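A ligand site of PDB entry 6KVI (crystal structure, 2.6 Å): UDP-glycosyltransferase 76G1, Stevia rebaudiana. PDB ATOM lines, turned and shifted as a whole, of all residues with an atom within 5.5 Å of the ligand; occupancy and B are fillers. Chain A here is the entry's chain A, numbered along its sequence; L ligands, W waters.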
ATOM      1  N   GLN A  24     -18.057  11.828  32.493  1.00  0.00           N
ATOM      2  CA  GLN A  24     -19.271  11.064  32.264  1.00  0.00           C
ATOM      3  C   GLN A  24     -19.153   9.702  32.920  1.00  0.00           C
ATOM      4  O   GLN A  24     -18.056   9.146  33.082  1.00  0.00           O
ATOM      5  CB  GLN A  24     -19.569  10.915  30.774  1.00  0.00           C
ATOM      6  CG  GLN A  24     -20.804  11.727  30.409  1.00  0.00           C
ATOM      7  CD  GLN A  24     -20.911  11.939  28.975  1.00  0.00           C
ATOM      8  OE1 GLN A  24     -21.026  13.061  28.497  1.00  0.00           O
ATOM      9  NE2 GLN A  24     -20.864  10.857  28.249  1.00  0.00           N
ATOM     10  N   GLY A  25     -20.268   9.162  33.322  1.00  0.00           N
ATOM     11  CA  GLY A  25     -20.232   8.082  34.258  1.00  0.00           C
ATOM     12  C   GLY A  25     -20.267   8.563  35.679  1.00  0.00           C
ATOM     13  O   GLY A  25     -20.738   7.828  36.555  1.00  0.00           O
ATOM     14  N   ASN A  28     -23.366  11.784  34.590  1.00  0.00           N
ATOM     15  CA  ASN A  28     -24.625  11.140  34.220  1.00  0.00           C
ATOM     16  C   ASN A  28     -25.454  10.708  35.423  1.00  0.00           C
ATOM     17  O   ASN A  28     -26.605  11.142  35.538  1.00  0.00           O
ATOM     18  CB  ASN A  28     -24.337   9.959  33.282  1.00  0.00           C
ATOM     19  CG  ASN A  28     -24.246  10.381  31.804  1.00  0.00           C
ATOM     20  OD1 ASN A  28     -24.432  11.557  31.456  1.00  0.00           O
ATOM     21  ND2 ASN A  28     -23.962   9.422  30.934  1.00  0.00           N
ATOM     22  N   ALA A 253     -29.625   9.428  30.497  1.00  0.00           N
ATOM     23  CA  ALA A 253     -28.620  10.422  30.846  1.00  0.00           C
ATOM     24  C   ALA A 253     -28.340  11.399  29.700  1.00  0.00           C
ATOM     25  O   ALA A 253     -27.316  12.089  29.744  1.00  0.00           O
ATOM     26  CB  ALA A 253     -27.326   9.753  31.283  1.00  0.00           C
ATOM     27  N   SER A 257     -24.889  14.618  28.193  1.00  0.00           N
ATOM     28  CA  SER A 257     -23.873  14.154  27.261  1.00  0.00           C
ATOM     29  C   SER A 257     -22.824  15.256  27.044  1.00  0.00           C
ATOM     30  O   SER A 257     -23.161  16.402  26.717  1.00  0.00           O
ATOM     31  CB  SER A 257     -24.516  13.760  25.943  1.00  0.00           C
ATOM     32  OG  SER A 257     -23.562  13.202  25.051  1.00  0.00           O
ATOM     33  N   HIS A 261     -24.525  14.044  20.043  1.00  0.00           N
ATOM     34  CA  HIS A 261     -25.135  12.787  19.636  1.00  0.00           C
ATOM     35  C   HIS A 261     -25.124  12.664  18.115  1.00  0.00           C
ATOM     36  O   HIS A 261     -25.645  13.533  17.414  1.00  0.00           O
ATOM     37  CB  HIS A 261     -26.569  12.706  20.140  1.00  0.00           C
ATOM     38  CG  HIS A 261     -26.685  12.531  21.616  1.00  0.00           C
ATOM     39  ND1 HIS A 261     -27.549  13.285  22.385  1.00  0.00           N
ATOM     40  CD2 HIS A 261     -26.025  11.719  22.477  1.00  0.00           C
ATOM     41  CE1 HIS A 261     -27.429  12.932  23.652  1.00  0.00           C
ATOM     42  NE2 HIS A 261     -26.510  11.989  23.736  1.00  0.00           N
ATOM     43  N   TYR A 279     -24.759  -3.783  19.590  1.00  0.00           N
ATOM     44  CA  TYR A 279     -24.256  -2.445  19.921  1.00  0.00           C
ATOM     45  C   TYR A 279     -22.904  -2.596  20.617  1.00  0.00           C
ATOM     46  O   TYR A 279     -22.736  -3.441  21.512  1.00  0.00           O
ATOM     47  CB  TYR A 279     -25.258  -1.676  20.769  1.00  0.00           C
ATOM     48  CG  TYR A 279     -24.764  -0.346  21.291  1.00  0.00           C
ATOM     49  CD1 TYR A 279     -24.478   0.724  20.419  1.00  0.00           C
ATOM     50  CD2 TYR A 279     -24.569  -0.144  22.660  1.00  0.00           C
ATOM     51  CE1 TYR A 279     -24.007   1.951  20.909  1.00  0.00           C
ATOM     52  CE2 TYR A 279     -24.102   1.075  23.153  1.00  0.00           C
ATOM     53  CZ  TYR A 279     -23.830   2.116  22.279  1.00  0.00           C
ATOM     54  OH  TYR A 279     -23.372   3.326  22.806  1.00  0.00           O
ATOM     55  N   SER A 281     -19.475  -0.553  22.335  1.00  0.00           N
ATOM     56  CA  SER A 281     -19.065   0.716  22.928  1.00  0.00           C
ATOM     57  C   SER A 281     -18.297   0.459  24.214  1.00  0.00           C
ATOM     58  O   SER A 281     -18.794  -0.236  25.099  1.00  0.00           O
ATOM     59  CB  SER A 281     -20.270   1.595  23.211  1.00  0.00           C
ATOM     60  OG  SER A 281     -19.883   2.709  23.987  1.00  0.00           O
ATOM     61  N   PHE A 282     -17.103   1.036  24.334  1.00  0.00           N
ATOM     62  CA  PHE A 282     -16.267   0.795  25.521  1.00  0.00           C
ATOM     63  C   PHE A 282     -16.143   2.027  26.419  1.00  0.00           C
ATOM     64  O   PHE A 282     -15.146   2.205  27.111  1.00  0.00           O
ATOM     65  CB  PHE A 282     -14.914   0.228  25.099  1.00  0.00           C
ATOM     66  CG  PHE A 282     -15.011  -1.042  24.275  1.00  0.00           C
ATOM     67  CD1 PHE A 282     -15.486  -2.227  24.828  1.00  0.00           C
ATOM     68  CD2 PHE A 282     -14.628  -1.059  22.940  1.00  0.00           C
ATOM     69  CE1 PHE A 282     -15.569  -3.400  24.078  1.00  0.00           C
ATOM     70  CE2 PHE A 282     -14.720  -2.231  22.179  1.00  0.00           C
ATOM     71  CZ  PHE A 282     -15.181  -3.406  22.750  1.00  0.00           C
ATOM     72  N   GLY A 283     -17.184   2.867  26.441  1.00  0.00           N
ATOM     73  CA  GLY A 283     -17.333   3.881  27.492  1.00  0.00           C
ATOM     74  C   GLY A 283     -16.824   5.251  27.102  1.00  0.00           C
ATOM     75  O   GLY A 283     -16.800   5.624  25.921  1.00  0.00           O
ATOM     76  N   SER A 284     -16.403   6.019  28.109  1.00  0.00           N
ATOM     77  CA  SER A 284     -15.988   7.400  27.862  1.00  0.00           C
ATOM     78  C   SER A 284     -14.483   7.616  27.954  1.00  0.00           C
ATOM     79  O   SER A 284     -14.017   8.676  27.512  1.00  0.00           O
ATOM     80  CB  SER A 284     -16.688   8.363  28.827  1.00  0.00           C
ATOM     81  OG  SER A 284     -16.263   8.200  30.171  1.00  0.00           O
ATOM     82  N   THR A 285     -13.710   6.664  28.480  1.00  0.00           N
ATOM     83  CA  THR A 285     -12.311   6.911  28.793  1.00  0.00           C
ATOM     84  C   THR A 285     -11.341   5.839  28.320  1.00  0.00           C
ATOM     85  O   THR A 285     -10.141   6.043  28.459  1.00  0.00           O
ATOM     86  CB  THR A 285     -12.084   7.085  30.317  1.00  0.00           C
ATOM     87  OG1 THR A 285     -11.397   5.932  30.843  1.00  0.00           O
ATOM     88  CG2 THR A 285     -13.386   7.238  31.084  1.00  0.00           C
ATOM     89  N   VAL A 310     -19.690   2.340  18.452  1.00  0.00           N
ATOM     90  CA  VAL A 310     -19.249   3.652  18.895  1.00  0.00           C
ATOM     91  C   VAL A 310     -17.751   3.553  19.136  1.00  0.00           C
ATOM     92  O   VAL A 310     -17.302   2.732  19.948  1.00  0.00           O
ATOM     93  CB  VAL A 310     -19.983   4.125  20.157  1.00  0.00           C
ATOM     94  CG1 VAL A 310     -19.404   5.456  20.635  1.00  0.00           C
ATOM     95  CG2 VAL A 310     -21.477   4.257  19.917  1.00  0.00           C
ATOM     96  N   LYS A 338     -19.057   8.337  16.387  1.00  0.00           N
ATOM     97  CA  LYS A 338     -18.289   8.862  17.508  1.00  0.00           C
ATOM     98  C   LYS A 338     -19.053   8.827  18.820  1.00  0.00           C
ATOM     99  O   LYS A 338     -18.422   8.773  19.878  1.00  0.00           O
ATOM    100  CB  LYS A 338     -17.832  10.301  17.253  1.00  0.00           C
ATOM    101  CG  LYS A 338     -17.760  10.698  15.814  1.00  0.00           C
ATOM    102  CD  LYS A 338     -16.346  10.967  15.389  1.00  0.00           C
ATOM    103  CE  LYS A 338     -16.357  11.519  13.965  1.00  0.00           C
ATOM    104  NZ  LYS A 338     -15.221  12.447  13.717  1.00  0.00           N
ATOM    105  N   TRP A 339     -20.390   8.852  18.768  1.00  0.00           N
ATOM    106  CA  TRP A 339     -21.157   9.038  19.992  1.00  0.00           C
ATOM    107  C   TRP A 339     -22.631   8.888  19.671  1.00  0.00           C
ATOM    108  O   TRP A 339     -23.071   9.281  18.592  1.00  0.00           O
ATOM    109  CB  TRP A 339     -20.836  10.420  20.572  1.00  0.00           C
ATOM    110  CG  TRP A 339     -21.196  10.600  21.983  1.00  0.00           C
ATOM    111  CD1 TRP A 339     -22.159  11.439  22.475  1.00  0.00           C
ATOM    112  CD2 TRP A 339     -20.610   9.945  23.110  1.00  0.00           C
ATOM    113  NE1 TRP A 339     -22.212  11.338  23.845  1.00  0.00           N
ATOM    114  CE2 TRP A 339     -21.268  10.427  24.263  1.00  0.00           C
ATOM    115  CE3 TRP A 339     -19.596   8.985  23.261  1.00  0.00           C
ATOM    116  CZ2 TRP A 339     -20.948   9.985  25.546  1.00  0.00           C
ATOM    117  CZ3 TRP A 339     -19.272   8.554  24.551  1.00  0.00           C
ATOM    118  CH2 TRP A 339     -19.952   9.049  25.669  1.00  0.00           C
ATOM    119  N   VAL A 340     -23.392   8.282  20.582  1.00  0.00           N
ATOM    120  CA  VAL A 340     -24.851   8.173  20.457  1.00  0.00           C
ATOM    121  C   VAL A 340     -25.487   8.503  21.803  1.00  0.00           C
ATOM    122  O   VAL A 340     -24.806   8.615  22.842  1.00  0.00           O
ATOM    123  CB  VAL A 340     -25.283   6.760  20.003  1.00  0.00           C
ATOM    124  CG1 VAL A 340     -24.754   6.433  18.635  1.00  0.00           C
ATOM    125  CG2 VAL A 340     -24.843   5.701  21.013  1.00  0.00           C
ATOM    126  N   PRO A 341     -26.800   8.667  21.824  1.00  0.00           N
ATOM    127  CA  PRO A 341     -27.538   8.608  23.102  1.00  0.00           C
ATOM    128  C   PRO A 341     -27.699   7.148  23.496  1.00  0.00           C
ATOM    129  O   PRO A 341     -28.609   6.469  22.999  1.00  0.00           O
ATOM    130  CB  PRO A 341     -28.890   9.256  22.766  1.00  0.00           C
ATOM    131  CG  PRO A 341     -28.799   9.715  21.329  1.00  0.00           C
ATOM    132  CD  PRO A 341     -27.693   8.943  20.690  1.00  0.00           C
ATOM    133  N   GLN A 342     -26.817   6.661  24.382  1.00  0.00           N
ATOM    134  CA  GLN A 342     -26.603   5.216  24.477  1.00  0.00           C
ATOM    135  C   GLN A 342     -27.859   4.485  24.969  1.00  0.00           C
ATOM    136  O   GLN A 342     -28.248   3.451  24.409  1.00  0.00           O
ATOM    137  CB  GLN A 342     -25.403   4.899  25.361  1.00  0.00           C
ATOM    138  CG  GLN A 342     -25.242   3.401  25.650  1.00  0.00           C
ATOM    139  CD  GLN A 342     -23.905   3.035  26.265  1.00  0.00           C
ATOM    140  OE1 GLN A 342     -22.850   3.362  25.720  1.00  0.00           O
ATOM    141  NE2 GLN A 342     -23.945   2.368  27.421  1.00  0.00           N
ATOM    142  N   GLN A 343     -28.508   4.998  26.009  1.00  0.00           N
ATOM    143  CA  GLN A 343     -29.638   4.236  26.541  1.00  0.00           C
ATOM    144  C   GLN A 343     -30.761   4.163  25.515  1.00  0.00           C
ATOM    145  O   GLN A 343     -31.360   3.100  25.299  1.00  0.00           O
ATOM    146  CB  GLN A 343     -30.134   4.803  27.867  1.00  0.00           C
ATOM    147  CG  GLN A 343     -30.939   3.739  28.625  1.00  0.00           C
ATOM    148  CD  GLN A 343     -31.457   4.215  29.958  1.00  0.00           C
ATOM    149  OE1 GLN A 343     -30.827   5.015  30.629  1.00  0.00           O
ATOM    150  NE2 GLN A 343     -32.609   3.714  30.348  1.00  0.00           N
ATOM    151  N   HIS A 357     -17.462  -2.404  27.624  1.00  0.00           N
ATOM    152  CA  HIS A 357     -16.327  -2.456  28.532  1.00  0.00           C
ATOM    153  C   HIS A 357     -16.751  -2.651  29.984  1.00  0.00           C
ATOM    154  O   HIS A 357     -15.885  -2.713  30.855  1.00  0.00           O
ATOM    155  CB  HIS A 357     -15.522  -1.157  28.423  1.00  0.00           C
ATOM    156  CG  HIS A 357     -16.119  -0.018  29.187  1.00  0.00           C
ATOM    157  ND1 HIS A 357     -17.414   0.420  28.988  1.00  0.00           N
ATOM    158  CD2 HIS A 357     -15.600   0.777  30.143  1.00  0.00           C
ATOM    159  CE1 HIS A 357     -17.654   1.432  29.800  1.00  0.00           C
ATOM    160  NE2 HIS A 357     -16.571   1.673  30.503  1.00  0.00           N
ATOM    161  N   SER A 358     -18.048  -2.721  30.265  1.00  0.00           N
ATOM    162  CA  SER A 358     -18.563  -3.075  31.579  1.00  0.00           C
ATOM    163  C   SER A 358     -18.484  -1.929  32.577  1.00  0.00           C
ATOM    164  O   SER A 358     -18.436  -2.194  33.777  1.00  0.00           O
ATOM    165  CB  SER A 358     -17.845  -4.279  32.182  1.00  0.00           C
ATOM    166  OG  SER A 358     -17.681  -5.323  31.246  1.00  0.00           O
ATOM    167  N   GLY A 359     -18.437  -0.675  32.121  1.00  0.00           N
ATOM    168  CA  GLY A 359     -18.613   0.448  33.023  1.00  0.00           C
ATOM    169  C   GLY A 359     -19.957   0.328  33.706  1.00  0.00           C
ATOM    170  O   GLY A 359     -20.902  -0.160  33.088  1.00  0.00           O
ATOM    171  N   TRP A 360     -20.079   0.750  34.979  1.00  0.00           N
ATOM    172  CA  TRP A 360     -21.294   0.422  35.704  1.00  0.00           C
ATOM    173  C   TRP A 360     -22.527   1.066  35.066  1.00  0.00           C
ATOM    174  O   TRP A 360     -23.587   0.436  35.003  1.00  0.00           O
ATOM    175  CB  TRP A 360     -21.178   0.792  37.180  1.00  0.00           C
ATOM    176  CG  TRP A 360     -22.408   0.386  37.970  1.00  0.00           C
ATOM    177  CD1 TRP A 360     -23.302   1.219  38.600  1.00  0.00           C
ATOM    178  CD2 TRP A 360     -22.912  -0.958  38.185  1.00  0.00           C
ATOM    179  NE1 TRP A 360     -24.302   0.493  39.204  1.00  0.00           N
ATOM    180  CE2 TRP A 360     -24.089  -0.844  38.963  1.00  0.00           C
ATOM    181  CE3 TRP A 360     -22.471  -2.232  37.818  1.00  0.00           C
ATOM    182  CZ2 TRP A 360     -24.824  -1.959  39.371  1.00  0.00           C
ATOM    183  CZ3 TRP A 360     -23.220  -3.333  38.212  1.00  0.00           C
ATOM    184  CH2 TRP A 360     -24.369  -3.190  38.980  1.00  0.00           C
ATOM    185  N   ASN A 361     -22.395   2.287  34.535  1.00  0.00           N
ATOM    186  CA  ASN A 361     -23.556   2.946  33.913  1.00  0.00           C
ATOM    187  C   ASN A 361     -24.027   2.172  32.688  1.00  0.00           C
ATOM    188  O   ASN A 361     -25.229   1.892  32.530  1.00  0.00           O
ATOM    189  CB  ASN A 361     -23.235   4.382  33.493  1.00  0.00           C
ATOM    190  CG  ASN A 361     -22.910   5.278  34.671  1.00  0.00           C
ATOM    191  OD1 ASN A 361     -21.740   5.515  34.978  1.00  0.00           O
ATOM    192  ND2 ASN A 361     -23.960   5.761  35.345  1.00  0.00           N
ATOM    193  N   SER A 362     -23.108   1.863  31.783  1.00  0.00           N
ATOM    194  CA  SER A 362     -23.485   1.072  30.626  1.00  0.00           C
ATOM    195  C   SER A 362     -24.145  -0.222  31.078  1.00  0.00           C
ATOM    196  O   SER A 362     -25.236  -0.575  30.607  1.00  0.00           O
ATOM    197  CB  SER A 362     -22.274   0.790  29.742  1.00  0.00           C
ATOM    198  OG  SER A 362     -21.893   1.981  29.084  1.00  0.00           O
ATOM    199  N   THR A 363     -23.515  -0.909  32.026  1.00  0.00           N
ATOM    200  CA  THR A 363     -24.032  -2.178  32.500  1.00  0.00           C
ATOM    201  C   THR A 363     -25.455  -2.023  33.027  1.00  0.00           C
ATOM    202  O   THR A 363     -26.347  -2.805  32.685  1.00  0.00           O
ATOM    203  CB  THR A 363     -23.110  -2.759  33.571  1.00  0.00           C
ATOM    204  OG1 THR A 363     -21.844  -3.048  32.982  1.00  0.00           O
ATOM    205  CG2 THR A 363     -23.707  -4.029  34.130  1.00  0.00           C
ATOM    206  N   GLU A 365     -27.588   0.317  32.305  1.00  0.00           N
ATOM    207  CA  GLU A 365     -28.489   0.709  31.229  1.00  0.00           C
ATOM    208  C   GLU A 365     -28.957  -0.509  30.432  1.00  0.00           C
ATOM    209  O   GLU A 365     -30.149  -0.682  30.179  1.00  0.00           O
ATOM    210  CB  GLU A 365     -27.797   1.730  30.327  1.00  0.00           C
ATOM    211  CG  GLU A 365     -27.713   3.121  30.948  1.00  0.00           C
ATOM    212  CD  GLU A 365     -26.507   3.916  30.467  1.00  0.00           C
ATOM    213  OE1 GLU A 365     -25.794   3.457  29.557  1.00  0.00           O
ATOM    214  OE2 GLU A 365     -26.286   5.017  31.029  1.00  0.00           O
ATOM    215  N   GLN A 382     -14.501  -2.656  36.455  1.00  0.00           N
ATOM    216  CA  GLN A 382     -15.034  -3.315  35.268  1.00  0.00           C
ATOM    217  C   GLN A 382     -14.875  -4.825  35.289  1.00  0.00           C
ATOM    218  O   GLN A 382     -15.851  -5.537  34.990  1.00  0.00           O
ATOM    219  CB  GLN A 382     -14.387  -2.695  34.019  1.00  0.00           C
ATOM    220  CG  GLN A 382     -14.604  -1.182  33.945  1.00  0.00           C
ATOM    221  CD  GLN A 382     -13.755  -0.508  32.877  1.00  0.00           C
ATOM    222  OE1 GLN A 382     -13.006  -1.164  32.152  1.00  0.00           O
ATOM    223  NE2 GLN A 382     -13.880   0.815  32.766  1.00  0.00           N
HETATM  224  N1  LIG L   1     -22.513   6.932  26.499  1.00  0.00           N
HETATM  225  C1  LIG L   1     -23.263   7.693  25.623  1.00  0.00           C
HETATM  226  N2  LIG L   1     -22.974   7.638  24.268  1.00  0.00           N
HETATM  227  C2  LIG L   1     -21.948   6.829  23.829  1.00  0.00           C
HETATM  228  C3  LIG L   1     -21.194   6.064  24.738  1.00  0.00           C
HETATM  229  C4  LIG L   1     -21.523   6.077  26.074  1.00  0.00           C
HETATM  230  O1  LIG L   1     -24.182   8.395  26.052  1.00  0.00           O
HETATM  231  O2  LIG L   1     -21.698   6.805  22.622  1.00  0.00           O
HETATM  232  C5  LIG L   1     -22.833   7.015  27.929  1.00  0.00           C
HETATM  233  C6  LIG L   1     -23.457   5.716  28.424  1.00  0.00           C
HETATM  234  O3  LIG L   1     -24.849   5.647  28.203  1.00  0.00           O
HETATM  235  C7  LIG L   1     -23.097   5.774  29.878  1.00  0.00           C
HETATM  236  C8  LIG L   1     -21.830   6.652  29.957  1.00  0.00           C
HETATM  237  O4  LIG L   1     -21.661   7.225  28.683  1.00  0.00           O
HETATM  238  O5  LIG L   1     -24.177   6.322  30.596  1.00  0.00           O
HETATM  239  C9  LIG L   1     -20.541   5.899  30.304  1.00  0.00           C
HETATM  240  O6  LIG L   1     -20.534   5.477  31.646  1.00  0.00           O
HETATM  241  P1  LIG L   1     -19.835   4.086  32.067  1.00  0.00           P
HETATM  242  O7  LIG L   1     -20.552   2.981  31.436  1.00  0.00           O
HETATM  243  O8  LIG L   1     -19.767   3.940  33.533  1.00  0.00           O
HETATM  244  O9  LIG L   1     -18.420   4.130  31.333  1.00  0.00           O
HETATM  245  P2  LIG L   1     -17.076   4.935  31.727  1.00  0.00           P
HETATM  246  O10 LIG L   1     -16.898   5.940  30.687  1.00  0.00           O
HETATM  247  O11 LIG L   1     -16.005   3.931  31.724  1.00  0.00           O
HETATM  248  O12 LIG L   1     -17.177   5.576  33.059  1.00  0.00           O
HETATM  249  O   HOH W   1     -25.960  10.031  25.940  1.00  0.00           O
HETATM  250  O   HOH W   2     -17.676   5.041  35.525  1.00  0.00           O
HETATM  251  O   HOH W   3     -27.192   7.003  28.190  1.00  0.00           O
HETATM  252  O   HOH W   4     -20.390   2.847  26.604  1.00  0.00           O
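Merely in contact with the ligand: Gln 24 (3.7 Å), Gly 25 (3.7 Å), Tyr 279 (3.9 Å), Ser 281 (3.7 Å), Gly 283 (3.7 Å), Thr 285 (3.8 Å), Val 310 (3.3 Å), Trp 339 (3.1 Å), Gly 359 (3.5 Å), Trp 360 (3.5 Å) and Gln 382 (3.9 Å). Hydrophobic or aromatic side chains that line the ligand: Val 310, Trp 339, Val 340 and His 357. 19 residues have an atom within 4 Å of the ligand: Gln 24, Gly 25, Asn 28, Tyr 279, Ser 281, Gly 283, Ser 284, Thr 285, Val 310, Trp 339, Val 340, Gln 342, His 357, Gly 359, Trp 360, Asn 361, Ser 362, Glu 365 and Gln 382.
A ring nitrogen (ND1) of His 357 sits close to the backbone carbonyl oxygen (O) of Phe 282 (3.4 Å). OG1 of Thr 363 sits at hydrogen-bond distance from O of Gly 359 (3.0 Å). OE1 of Gln 342 sits at hydrogen-bond distance from OH of Tyr 279 (3.0 Å). NE1 of Trp 339 lies within hydrogen-bond range of OG of Ser 257 (2.6 Å). OG of Ser 362 lies within hydrogen-bond range of NE2 of Gln 342, 2.7 Å away. NE2 of Gln 342 is in hydrogen-bond range of OE1 of Glu 365. OE1 of Gln 342 is in hydrogen-bond range of OG of Ser 281, at 3.5 Å. The backbone carbonyl oxygen (O) of Gly 25 lies close to the side-chain amide oxygen (OD1) of Asn 361 (3.0 Å).
The side-chain hydroxyl (OG) of Ser 362 is in hydrogen-bond range of an oxygen (O7) of the ligand, 2.9 Å away. OG of Ser 284 is in hydrogen-bond range of O10 of the ligand, at 2.4 Å. The backbone carbonyl oxygen (O) of Val 340 is in hydrogen-bond range of a nitrogen (N2) of the ligand (2.5 Å). The side-chain amide nitrogen of Asn 28 is in hydrogen-bond range of an oxygen (O5) of the ligand (3.1 Å). The backbone NH (N) of Ser 362 sits at hydrogen-bond distance from an oxygen (O7) of the ligand (2.8 Å). NE2 of Gln 342 sits close to O3 of the ligand (3.5 Å). The backbone NH (N) of Asn 361 is in hydrogen-bond range of an oxygen (O8) of the ligand, at 3.3 Å. OD1 of Asn 361 sits close to O8 of the ligand, 2.9 Å away. An oxygen (O10) of the ligand lies within hydrogen-bond range of the backbone NH (N) of Ser 284 (2.6 Å). An oxygen (O5) of the ligand sits at hydrogen-bond distance from the side-chain carboxylate of Glu 365, 2.5 Å away. O11 of the ligand sits at hydrogen-bond distance from NE2 of His 357, 2.6 Å away. The backbone NH (N) of Val 340 sits at hydrogen-bond distance from an oxygen (O2) of the ligand, 3.0 Å away.
Water W1 bridges O1 of the ligand (2.4 Å) and NE2 of His 261 (3.0 Å). Water W3 bridges an oxygen (O3) of the ligand (2.7 Å) and the backbone NH of Gln 343 (3.2 Å). Water W4 lies within hydrogen-bond range of the side-chain amide oxygen (OE1) of Gln 342 (2.7 Å), the side-chain hydroxyl (OG) of Ser 281 (2.7 Å), the side-chain hydroxyl (OG) of Ser 362 (3.0 Å) and the backbone NH (N) of Gly 283 (3.2 Å).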
